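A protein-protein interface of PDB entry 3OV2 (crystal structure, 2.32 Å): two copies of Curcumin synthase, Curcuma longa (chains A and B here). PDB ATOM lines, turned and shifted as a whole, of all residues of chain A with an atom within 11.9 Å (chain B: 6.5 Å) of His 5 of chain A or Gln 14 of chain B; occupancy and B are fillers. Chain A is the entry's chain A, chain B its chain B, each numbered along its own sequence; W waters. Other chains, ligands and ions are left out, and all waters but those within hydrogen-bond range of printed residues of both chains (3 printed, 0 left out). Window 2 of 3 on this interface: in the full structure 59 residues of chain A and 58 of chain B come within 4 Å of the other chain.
Water W3 bridges the side-chain carboxylate (OD1) of Asp 227 of chain B (2.6 Å) and a ring nitrogen (NE2) of His 5 of chain A (3.0 Å).
Water W1 lies within hydrogen-bond range of the guanidinium group (NH1) of Arg 12 of chain B, the backbone carbonyl oxygen (O) of Glu 179 of chain A and the backbone carbonyl oxygen (O) of Ala 13 of chain A.
Water W2 bridges OD1 of Asn 180 of chain A and NH2 of Arg 12 of chain B.
His 5 of chain A touches just these residues of chain B: Gln 14 and Gly 15.
Of the printed residues of chain A, Gln 14 of chain B touches His 5, Arg 8 and Arg 12.
Of chain A, only His 5 (3.6 Å) and Arg 8 (3.9 Å) come within 4 Å of Gly 15 of chain B.
Pro 16 of chain B touches two residues of chain A.
Of chain A, only Arg 8 (3.0 Å) and Asn 180 (3.0 Å) come within 4 Å of Glu 179 of chain B.
No residue of chain A comes within 4 Å of Ala 226 of chain B.
No residue of chain A comes within 4 Å of Asp 227 of chain B.
Printed residues of chain A within 4 Å of Glu 238 of chain B: Leu 4.
Of the printed residues of chain B, Glu 179 of chain A touches Arg 12 (3.1 Å).
Of the printed residues of chain B, Leu 4 of chain A touches Pro 16 (3.8 Å) and Glu 238 (3.2 Å).
Arg 12 of chain A touches its own counterpart, Arg 12 of chain B.
Arg 12 of chain A touches Ala 13 of chain B, and with the chains exchanged Ala 13 of chain A touches Arg 12 of chain B.
Glu 179 of chain A touches Arg 12 of chain B, but with the chains exchanged Arg 12 of chain A does not touch Glu 179 of chain B (5.5 Å).
Of the 14 pairs that touch across the chains among the printed residues, 3 have their exchanged pair printed and touching as well.
Hydrophobic or aromatic side chains of chain B within 4 Å of the printed part of chain A: Pro 16.
Printed residues of chain A that touch a printed residue of chain B: Leu 4, His 5, Arg 8, Arg 12, Ala 13, Glu 179 and Asn 180.
Hydrophobic or aromatic side chains of chain A within 4 Å of the printed part of chain B: Leu 4 and His 5.
Among the printed residues, Asp or Glu carboxylates within 4 Å of a Lys or Arg side-chain nitrogen of the other chain: Arg 8 of chain A with Glu 179 of chain B.
The backbone carbonyl oxygen of Glu 179 of chain A sits at hydrogen-bond distance from the guanidinium group of Arg 12 of chain B.
The side-chain amide nitrogen of Asn 180 of chain A lies within hydrogen-bond range of the side-chain carboxylate of Glu 179 of chain B, at 3.0 Å.
The guanidinium group of Arg 12 of chain A lies within hydrogen-bond range of the backbone carbonyl oxygen of Ala 13 of chain B (3.2 Å).
O of Ala 13 of chain A sits at hydrogen-bond distance from NH2 of Arg 12 of chain B, 2.9 Å away.
NH2 of Arg 12 of chain A is in hydrogen-bond range of O of Gln 14 of chain B.
OE1 of Glu 179 of chain B is in salt-bridge range of NE of Arg 8 of chain A.
Among the printed residues, merely in contact across the chains: Leu 4 of chain A with Glu 238 of chain B (3.2 Å), Arg 12 of chain A with Arg 12 of chain B (3.5 Å), His 5 of chain A with Gly 15 of chain B (3.6 Å), His 5 of chain A with Gln 14 of chain B (3.7 Å), Arg 8 of chain A with Gln 14 of chain B (3.8 Å), Leu 4 of chain A with Pro 16 of chain B (3.8 Å), Arg 8 of chain A with Pro 16 of chain B (3.9 Å) and Arg 8 of chain A with Gly 15 of chain B (3.9 Å).
N of His 5 of chain A sits close to ND2 of Asn 3 of chain A, 3.3 Å away.
N of Ala 13 of chain B lies close to O of Glu 179 of chain B, 3.2 Å away.
The side-chain carboxylate of Asp 227 of chain B sits at hydrogen-bond distance from the backbone NH of Gln 14 of chain B (2.9 Å).
N of Gly 15 of chain B lies within hydrogen-bond range of OD1 of Asp 227 of chain B, at 2.8 Å.
The backbone NH (N) of Ala 13 of chain A lies within hydrogen-bond range of the backbone carbonyl oxygen (O) of Glu 179 of chain A.
The side-chain amide oxygen (OD1) of Asn 180 of chain A sits at hydrogen-bond distance from the guanidinium group (NH1) of Arg 8 of chain A, 2.8 Å away.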
ATOM      1  N   ASN A   3     -12.235  12.152 -15.019  1.00  0.00           N
ATOM      2  CA  ASN A   3     -12.923  11.193 -14.104  1.00  0.00           C
ATOM      3  C   ASN A   3     -12.753  11.629 -12.646  1.00  0.00           C
ATOM      4  O   ASN A   3     -11.627  11.776 -12.167  1.00  0.00           O
ATOM      5  CB  ASN A   3     -12.397   9.762 -14.336  1.00  0.00           C
ATOM      6  CG  ASN A   3     -13.247   8.674 -13.648  1.00  0.00           C
ATOM      7  OD1 ASN A   3     -12.970   7.483 -13.807  1.00  0.00           O
ATOM      8  ND2 ASN A   3     -14.269   9.073 -12.897  1.00  0.00           N
ATOM      9  N   LEU A   4     -13.888  11.848 -11.972  1.00  0.00           N
ATOM     10  CA  LEU A   4     -13.962  12.252 -10.552  1.00  0.00           C
ATOM     11  C   LEU A   4     -13.437  11.213  -9.537  1.00  0.00           C
ATOM     12  O   LEU A   4     -12.854  11.584  -8.517  1.00  0.00           O
ATOM     13  CB  LEU A   4     -15.406  12.670 -10.181  1.00  0.00           C
ATOM     14  CG  LEU A   4     -16.555  11.640 -10.278  1.00  0.00           C
ATOM     15  CD1 LEU A   4     -17.683  11.957  -9.297  1.00  0.00           C
ATOM     16  CD2 LEU A   4     -17.114  11.441 -11.714  1.00  0.00           C
ATOM     17  N   HIS A   5     -13.664   9.926  -9.806  1.00  0.00           N
ATOM     18  CA  HIS A   5     -13.258   8.855  -8.891  1.00  0.00           C
ATOM     19  C   HIS A   5     -11.817   8.403  -9.131  1.00  0.00           C
ATOM     20  O   HIS A   5     -11.088   8.141  -8.174  1.00  0.00           O
ATOM     21  CB  HIS A   5     -14.209   7.658  -8.987  1.00  0.00           C
ATOM     22  CG  HIS A   5     -15.500   7.841  -8.249  1.00  0.00           C
ATOM     23  ND1 HIS A   5     -16.482   8.714  -8.668  1.00  0.00           N
ATOM     24  CD2 HIS A   5     -15.982   7.242  -7.133  1.00  0.00           C
ATOM     25  CE1 HIS A   5     -17.507   8.655  -7.836  1.00  0.00           C
ATOM     26  NE2 HIS A   5     -17.232   7.766  -6.897  1.00  0.00           N
ATOM     27  N   ALA A   6     -11.423   8.307 -10.404  1.00  0.00           N
ATOM     28  CA  ALA A   6     -10.051   7.961 -10.787  1.00  0.00           C
ATOM     29  C   ALA A   6      -9.047   8.989 -10.272  1.00  0.00           C
ATOM     30  O   ALA A   6      -8.050   8.615  -9.653  1.00  0.00           O
ATOM     31  CB  ALA A   6      -9.929   7.801 -12.305  1.00  0.00           C
ATOM     32  N   LEU A   7      -9.316  10.274 -10.535  1.00  0.00           N
ATOM     33  CA  LEU A   7      -8.528  11.393  -9.980  1.00  0.00           C
ATOM     34  C   LEU A   7      -8.407  11.283  -8.448  1.00  0.00           C
ATOM     35  O   LEU A   7      -7.324  11.449  -7.890  1.00  0.00           O
ATOM     36  CB  LEU A   7      -9.118  12.757 -10.404  1.00  0.00           C
ATOM     37  CG  LEU A   7      -8.688  14.071  -9.713  1.00  0.00           C
ATOM     38  CD1 LEU A   7      -8.489  15.223 -10.699  1.00  0.00           C
ATOM     39  CD2 LEU A   7      -9.654  14.493  -8.606  1.00  0.00           C
ATOM     40  N   ARG A   8      -9.523  10.986  -7.788  1.00  0.00           N
ATOM     41  CA  ARG A   8      -9.544  10.812  -6.340  1.00  0.00           C
ATOM     42  C   ARG A   8      -8.593   9.681  -5.914  1.00  0.00           C
ATOM     43  O   ARG A   8      -7.789   9.870  -4.997  1.00  0.00           O
ATOM     44  CB  ARG A   8     -10.988  10.581  -5.853  1.00  0.00           C
ATOM     45  CG  ARG A   8     -11.257  10.794  -4.363  1.00  0.00           C
ATOM     46  CD  ARG A   8     -11.439  12.275  -3.936  1.00  0.00           C
ATOM     47  NE  ARG A   8     -10.174  12.960  -3.623  1.00  0.00           N
ATOM     48  CZ  ARG A   8      -9.320  12.596  -2.663  1.00  0.00           C
ATOM     49  NH1 ARG A   8      -9.569  11.533  -1.907  1.00  0.00           N
ATOM     50  NH2 ARG A   8      -8.207  13.294  -2.464  1.00  0.00           N
ATOM     51  N   ARG A   9      -8.657   8.537  -6.604  1.00  0.00           N
ATOM     52  CA  ARG A   9      -7.844   7.356  -6.253  1.00  0.00           C
ATOM     53  C   ARG A   9      -6.341   7.615  -6.363  1.00  0.00           C
ATOM     54  O   ARG A   9      -5.550   7.000  -5.644  1.00  0.00           O
ATOM     55  CB  ARG A   9      -8.215   6.130  -7.108  1.00  0.00           C
ATOM     56  CG  ARG A   9      -9.669   5.627  -6.982  1.00  0.00           C
ATOM     57  CD  ARG A   9      -9.849   4.121  -7.311  1.00  0.00           C
ATOM     58  NE  ARG A   9      -9.334   3.739  -8.632  1.00  0.00           N
ATOM     59  CZ  ARG A   9      -8.146   3.166  -8.845  1.00  0.00           C
ATOM     60  NH1 ARG A   9      -7.765   2.862 -10.080  1.00  0.00           N
ATOM     61  NH2 ARG A   9      -7.333   2.900  -7.829  1.00  0.00           N
ATOM     62  N   GLU A  10      -5.954   8.521  -7.259  1.00  0.00           N
ATOM     63  CA  GLU A  10      -4.543   8.840  -7.488  1.00  0.00           C
ATOM     64  C   GLU A  10      -3.981   9.911  -6.522  1.00  0.00           C
ATOM     65  O   GLU A  10      -2.814   9.840  -6.119  1.00  0.00           O
ATOM     66  CB  GLU A  10      -4.329   9.244  -8.955  1.00  0.00           C
ATOM     67  CG  GLU A  10      -4.493   8.071  -9.955  1.00  0.00           C
ATOM     68  CD  GLU A  10      -4.767   8.512 -11.403  1.00  0.00           C
ATOM     69  OE1 GLU A  10      -4.952   9.725 -11.653  1.00  0.00           O
ATOM     70  OE2 GLU A  10      -4.800   7.634 -12.297  1.00  0.00           O
ATOM     71  N   GLN A  11      -4.822  10.877  -6.144  1.00  0.00           N
ATOM     72  CA  GLN A  11      -4.403  12.014  -5.313  1.00  0.00           C
ATOM     73  C   GLN A  11      -4.325  11.742  -3.801  1.00  0.00           C
ATOM     74  O   GLN A  11      -3.718  12.518  -3.074  1.00  0.00           O
ATOM     75  CB  GLN A  11      -5.302  13.245  -5.553  1.00  0.00           C
ATOM     76  CG  GLN A  11      -5.484  13.711  -7.024  1.00  0.00           C
ATOM     77  CD  GLN A  11      -4.239  14.346  -7.669  1.00  0.00           C
ATOM     78  OE1 GLN A  11      -3.124  14.286  -7.134  1.00  0.00           O
ATOM     79  NE2 GLN A  11      -4.438  14.952  -8.836  1.00  0.00           N
ATOM     80  N   ARG A  12      -4.940  10.665  -3.323  1.00  0.00           N
ATOM     81  CA  ARG A  12      -4.969  10.396  -1.879  1.00  0.00           C
ATOM     82  C   ARG A  12      -3.827   9.487  -1.404  1.00  0.00           C
ATOM     83  O   ARG A  12      -3.249   8.740  -2.192  1.00  0.00           O
ATOM     84  CB  ARG A  12      -6.338   9.858  -1.443  1.00  0.00           C
ATOM     85  CG  ARG A  12      -6.675   8.482  -1.970  1.00  0.00           C
ATOM     86  CD  ARG A  12      -8.165   8.170  -1.814  1.00  0.00           C
ATOM     87  NE  ARG A  12      -8.461   6.819  -2.289  1.00  0.00           N
ATOM     88  CZ  ARG A  12      -9.686   6.321  -2.475  1.00  0.00           C
ATOM     89  NH1 ARG A  12      -9.831   5.069  -2.915  1.00  0.00           N
ATOM     90  NH2 ARG A  12     -10.766   7.066  -2.227  1.00  0.00           N
ATOM     91  N   ALA A  13      -3.495   9.570  -0.119  1.00  0.00           N
ATOM     92  CA  ALA A  13      -2.466   8.695   0.454  1.00  0.00           C
ATOM     93  C   ALA A  13      -3.007   7.281   0.678  1.00  0.00           C
ATOM     94  O   ALA A  13      -4.216   7.070   0.705  1.00  0.00           O
ATOM     95  CB  ALA A  13      -1.917   9.282   1.750  1.00  0.00           C
ATOM     96  N   GLU A 179      -3.905  11.796   5.346  1.00  0.00           N
ATOM     97  CA  GLU A 179      -4.377  10.536   4.754  1.00  0.00           C
ATOM     98  C   GLU A 179      -5.025  10.766   3.400  1.00  0.00           C
ATOM     99  O   GLU A 179      -4.947   9.904   2.529  1.00  0.00           O
ATOM    100  CB  GLU A 179      -5.327   9.789   5.698  1.00  0.00           C
ATOM    101  CG  GLU A 179      -4.568   9.138   6.811  1.00  0.00           C
ATOM    102  CD  GLU A 179      -5.404   8.636   7.979  1.00  0.00           C
ATOM    103  OE1 GLU A 179      -6.673   8.758   7.996  1.00  0.00           O
ATOM    104  OE2 GLU A 179      -4.742   8.123   8.903  1.00  0.00           O
ATOM    105  N   ASN A 180      -5.640  11.938   3.239  1.00  0.00           N
ATOM    106  CA  ASN A 180      -6.414  12.257   2.052  1.00  0.00           C
ATOM    107  C   ASN A 180      -5.612  12.874   0.920  1.00  0.00           C
ATOM    108  O   ASN A 180      -6.125  13.059  -0.169  1.00  0.00           O
ATOM    109  CB  ASN A 180      -7.617  13.175   2.385  1.00  0.00           C
ATOM    110  CG  ASN A 180      -8.660  13.170   1.279  1.00  0.00           C
ATOM    111  OD1 ASN A 180      -9.109  12.105   0.837  1.00  0.00           O
ATOM    112  ND2 ASN A 180      -9.023  14.346   0.801  1.00  0.00           N
ATOM    113  N   ASN A 181      -4.356  13.200   1.178  1.00  0.00           N
ATOM    114  CA  ASN A 181      -3.523  13.844   0.164  1.00  0.00           C
ATOM    115  C   ASN A 181      -2.183  13.132   0.006  1.00  0.00           C
ATOM    116  O   ASN A 181      -1.344  13.183   0.905  1.00  0.00           O
ATOM    117  CB  ASN A 181      -3.303  15.308   0.539  1.00  0.00           C
ATOM    118  CG  ASN A 181      -4.587  16.077   0.603  1.00  0.00           C
ATOM    119  OD1 ASN A 181      -5.096  16.524  -0.424  1.00  0.00           O
ATOM    120  ND2 ASN A 181      -5.137  16.230   1.804  1.00  0.00           N
ATOM    121  N   ARG B  12     -12.350   4.891   4.893  1.00  0.00           N
ATOM    122  CA  ARG B  12     -12.264   6.093   4.056  1.00  0.00           C
ATOM    123  C   ARG B  12     -13.432   6.154   3.075  1.00  0.00           C
ATOM    124  O   ARG B  12     -14.059   5.140   2.776  1.00  0.00           O
ATOM    125  CB  ARG B  12     -10.916   6.170   3.321  1.00  0.00           C
ATOM    126  CG  ARG B  12     -10.797   5.227   2.126  1.00  0.00           C
ATOM    127  CD  ARG B  12      -9.352   5.025   1.709  1.00  0.00           C
ATOM    128  NE  ARG B  12      -8.696   6.308   1.465  1.00  0.00           N
ATOM    129  CZ  ARG B  12      -7.399   6.547   1.649  1.00  0.00           C
ATOM    130  NH1 ARG B  12      -6.594   5.569   2.083  1.00  0.00           N
ATOM    131  NH2 ARG B  12      -6.911   7.758   1.399  1.00  0.00           N
ATOM    132  N   ALA B  13     -13.732   7.351   2.597  1.00  0.00           N
ATOM    133  CA  ALA B  13     -14.799   7.538   1.619  1.00  0.00           C
ATOM    134  C   ALA B  13     -14.280   7.187   0.225  1.00  0.00           C
ATOM    135  O   ALA B  13     -13.076   7.086   0.027  1.00  0.00           O
ATOM    136  CB  ALA B  13     -15.325   8.981   1.670  1.00  0.00           C
ATOM    137  N   GLN B  14     -15.195   7.020  -0.728  1.00  0.00           N
ATOM    138  CA  GLN B  14     -14.849   6.607  -2.086  1.00  0.00           C
ATOM    139  C   GLN B  14     -14.745   7.795  -3.078  1.00  0.00           C
ATOM    140  O   GLN B  14     -13.705   7.999  -3.719  1.00  0.00           O
ATOM    141  CB  GLN B  14     -15.828   5.508  -2.569  1.00  0.00           C
ATOM    142  CG  GLN B  14     -15.778   5.169  -4.078  1.00  0.00           C
ATOM    143  CD  GLN B  14     -14.975   3.892  -4.417  1.00  0.00           C
ATOM    144  OE1 GLN B  14     -13.824   3.960  -4.891  1.00  0.00           O
ATOM    145  NE2 GLN B  14     -15.592   2.727  -4.195  1.00  0.00           N
ATOM    146  N   GLY B  15     -15.805   8.587  -3.175  1.00  0.00           N
ATOM    147  CA  GLY B  15     -15.863   9.681  -4.131  1.00  0.00           C
ATOM    148  C   GLY B  15     -15.382  11.034  -3.621  1.00  0.00           C
ATOM    149  O   GLY B  15     -14.867  11.142  -2.519  1.00  0.00           O
ATOM    150  N   PRO B  16     -15.541  12.080  -4.443  1.00  0.00           N
ATOM    151  CA  PRO B  16     -15.120  13.402  -3.999  1.00  0.00           C
ATOM    152  C   PRO B  16     -16.164  14.051  -3.082  1.00  0.00           C
ATOM    153  O   PRO B  16     -17.336  13.675  -3.111  1.00  0.00           O
ATOM    154  CB  PRO B  16     -14.999  14.183  -5.316  1.00  0.00           C
ATOM    155  CG  PRO B  16     -16.065  13.541  -6.219  1.00  0.00           C
ATOM    156  CD  PRO B  16     -16.150  12.094  -5.792  1.00  0.00           C
ATOM    157  N   ALA B 178     -14.663  15.119   4.661  1.00  0.00           N
ATOM    158  CA  ALA B 178     -15.660  14.290   3.994  1.00  0.00           C
ATOM    159  C   ALA B 178     -15.019  13.111   3.240  1.00  0.00           C
ATOM    160  O   ALA B 178     -15.478  11.982   3.343  1.00  0.00           O
ATOM    161  CB  ALA B 178     -16.519  15.130   3.061  1.00  0.00           C
ATOM    162  N   GLU B 179     -13.957  13.390   2.494  1.00  0.00           N
ATOM    163  CA  GLU B 179     -13.287  12.385   1.669  1.00  0.00           C
ATOM    164  C   GLU B 179     -12.542  11.293   2.457  1.00  0.00           C
ATOM    165  O   GLU B 179     -12.432  10.161   1.985  1.00  0.00           O
ATOM    166  CB  GLU B 179     -12.354  13.064   0.642  1.00  0.00           C
ATOM    167  CG  GLU B 179     -13.147  13.806  -0.424  1.00  0.00           C
ATOM    168  CD  GLU B 179     -12.317  14.630  -1.402  1.00  0.00           C
ATOM    169  OE1 GLU B 179     -11.072  14.693  -1.298  1.00  0.00           O
ATOM    170  OE2 GLU B 179     -12.943  15.236  -2.295  1.00  0.00           O
ATOM    171  N   ARG B 182     -15.660   7.568   5.590  1.00  0.00           N
ATOM    172  CA  ARG B 182     -16.871   7.012   5.006  1.00  0.00           C
ATOM    173  C   ARG B 182     -18.063   7.404   5.857  1.00  0.00           C
ATOM    174  O   ARG B 182     -18.060   7.189   7.073  1.00  0.00           O
ATOM    175  CB  ARG B 182     -16.766   5.481   4.903  1.00  0.00           C
ATOM    176  CG  ARG B 182     -17.975   4.797   4.258  1.00  0.00           C
ATOM    177  CD  ARG B 182     -17.770   3.299   4.164  1.00  0.00           C
ATOM    178  NE  ARG B 182     -17.362   2.735   5.456  1.00  0.00           N
ATOM    179  CZ  ARG B 182     -18.145   2.021   6.269  1.00  0.00           C
ATOM    180  NH1 ARG B 182     -19.411   1.744   5.936  1.00  0.00           N
ATOM    181  NH2 ARG B 182     -17.654   1.567   7.419  1.00  0.00           N
ATOM    182  N   ALA B 226     -19.144  13.113   0.914  1.00  0.00           N
ATOM    183  CA  ALA B 226     -18.861  12.256  -0.227  1.00  0.00           C
ATOM    184  C   ALA B 226     -19.831  11.085  -0.235  1.00  0.00           C
ATOM    185  O   ALA B 226     -20.480  10.783   0.793  1.00  0.00           O
ATOM    186  CB  ALA B 226     -17.436  11.746  -0.163  1.00  0.00           C
ATOM    187  N   ASP B 227     -19.914  10.416  -1.387  1.00  0.00           N
ATOM    188  CA  ASP B 227     -20.739   9.208  -1.543  1.00  0.00           C
ATOM    189  C   ASP B 227     -22.204   9.537  -1.234  1.00  0.00           C
ATOM    190  O   ASP B 227     -22.770   9.014  -0.285  1.00  0.00           O
ATOM    191  CB  ASP B 227     -20.205   8.060  -0.656  1.00  0.00           C
ATOM    192  CG  ASP B 227     -18.719   7.750  -0.922  1.00  0.00           C
ATOM    193  OD1 ASP B 227     -18.282   7.879  -2.091  1.00  0.00           O
ATOM    194  OD2 ASP B 227     -17.989   7.378   0.032  1.00  0.00           O
ATOM    195  N   GLU B 238     -19.570  19.345  -6.976  1.00  0.00           N
ATOM    196  CA  GLU B 238     -18.466  18.514  -6.542  1.00  0.00           C
ATOM    197  C   GLU B 238     -17.248  19.409  -6.272  1.00  0.00           C
ATOM    198  O   GLU B 238     -16.928  20.327  -7.052  1.00  0.00           O
ATOM    199  CB  GLU B 238     -18.162  17.423  -7.566  1.00  0.00           C
ATOM    200  CG  GLU B 238     -19.379  16.502  -7.866  1.00  0.00           C
ATOM    201  CD  GLU B 238     -19.040  15.261  -8.686  1.00  0.00           C
ATOM    202  OE1 GLU B 238     -17.928  15.196  -9.255  1.00  0.00           O
ATOM    203  OE2 GLU B 238     -19.887  14.342  -8.762  1.00  0.00           O
HETATM  204  O   HOH W   1      -4.900   7.046   3.741  1.00  0.00           O
HETATM  205  O   HOH W   2      -8.816   9.713   2.265  1.00  0.00           O
HETATM  206  O   HOH W   3     -18.962   7.170  -4.529  1.00  0.00           O
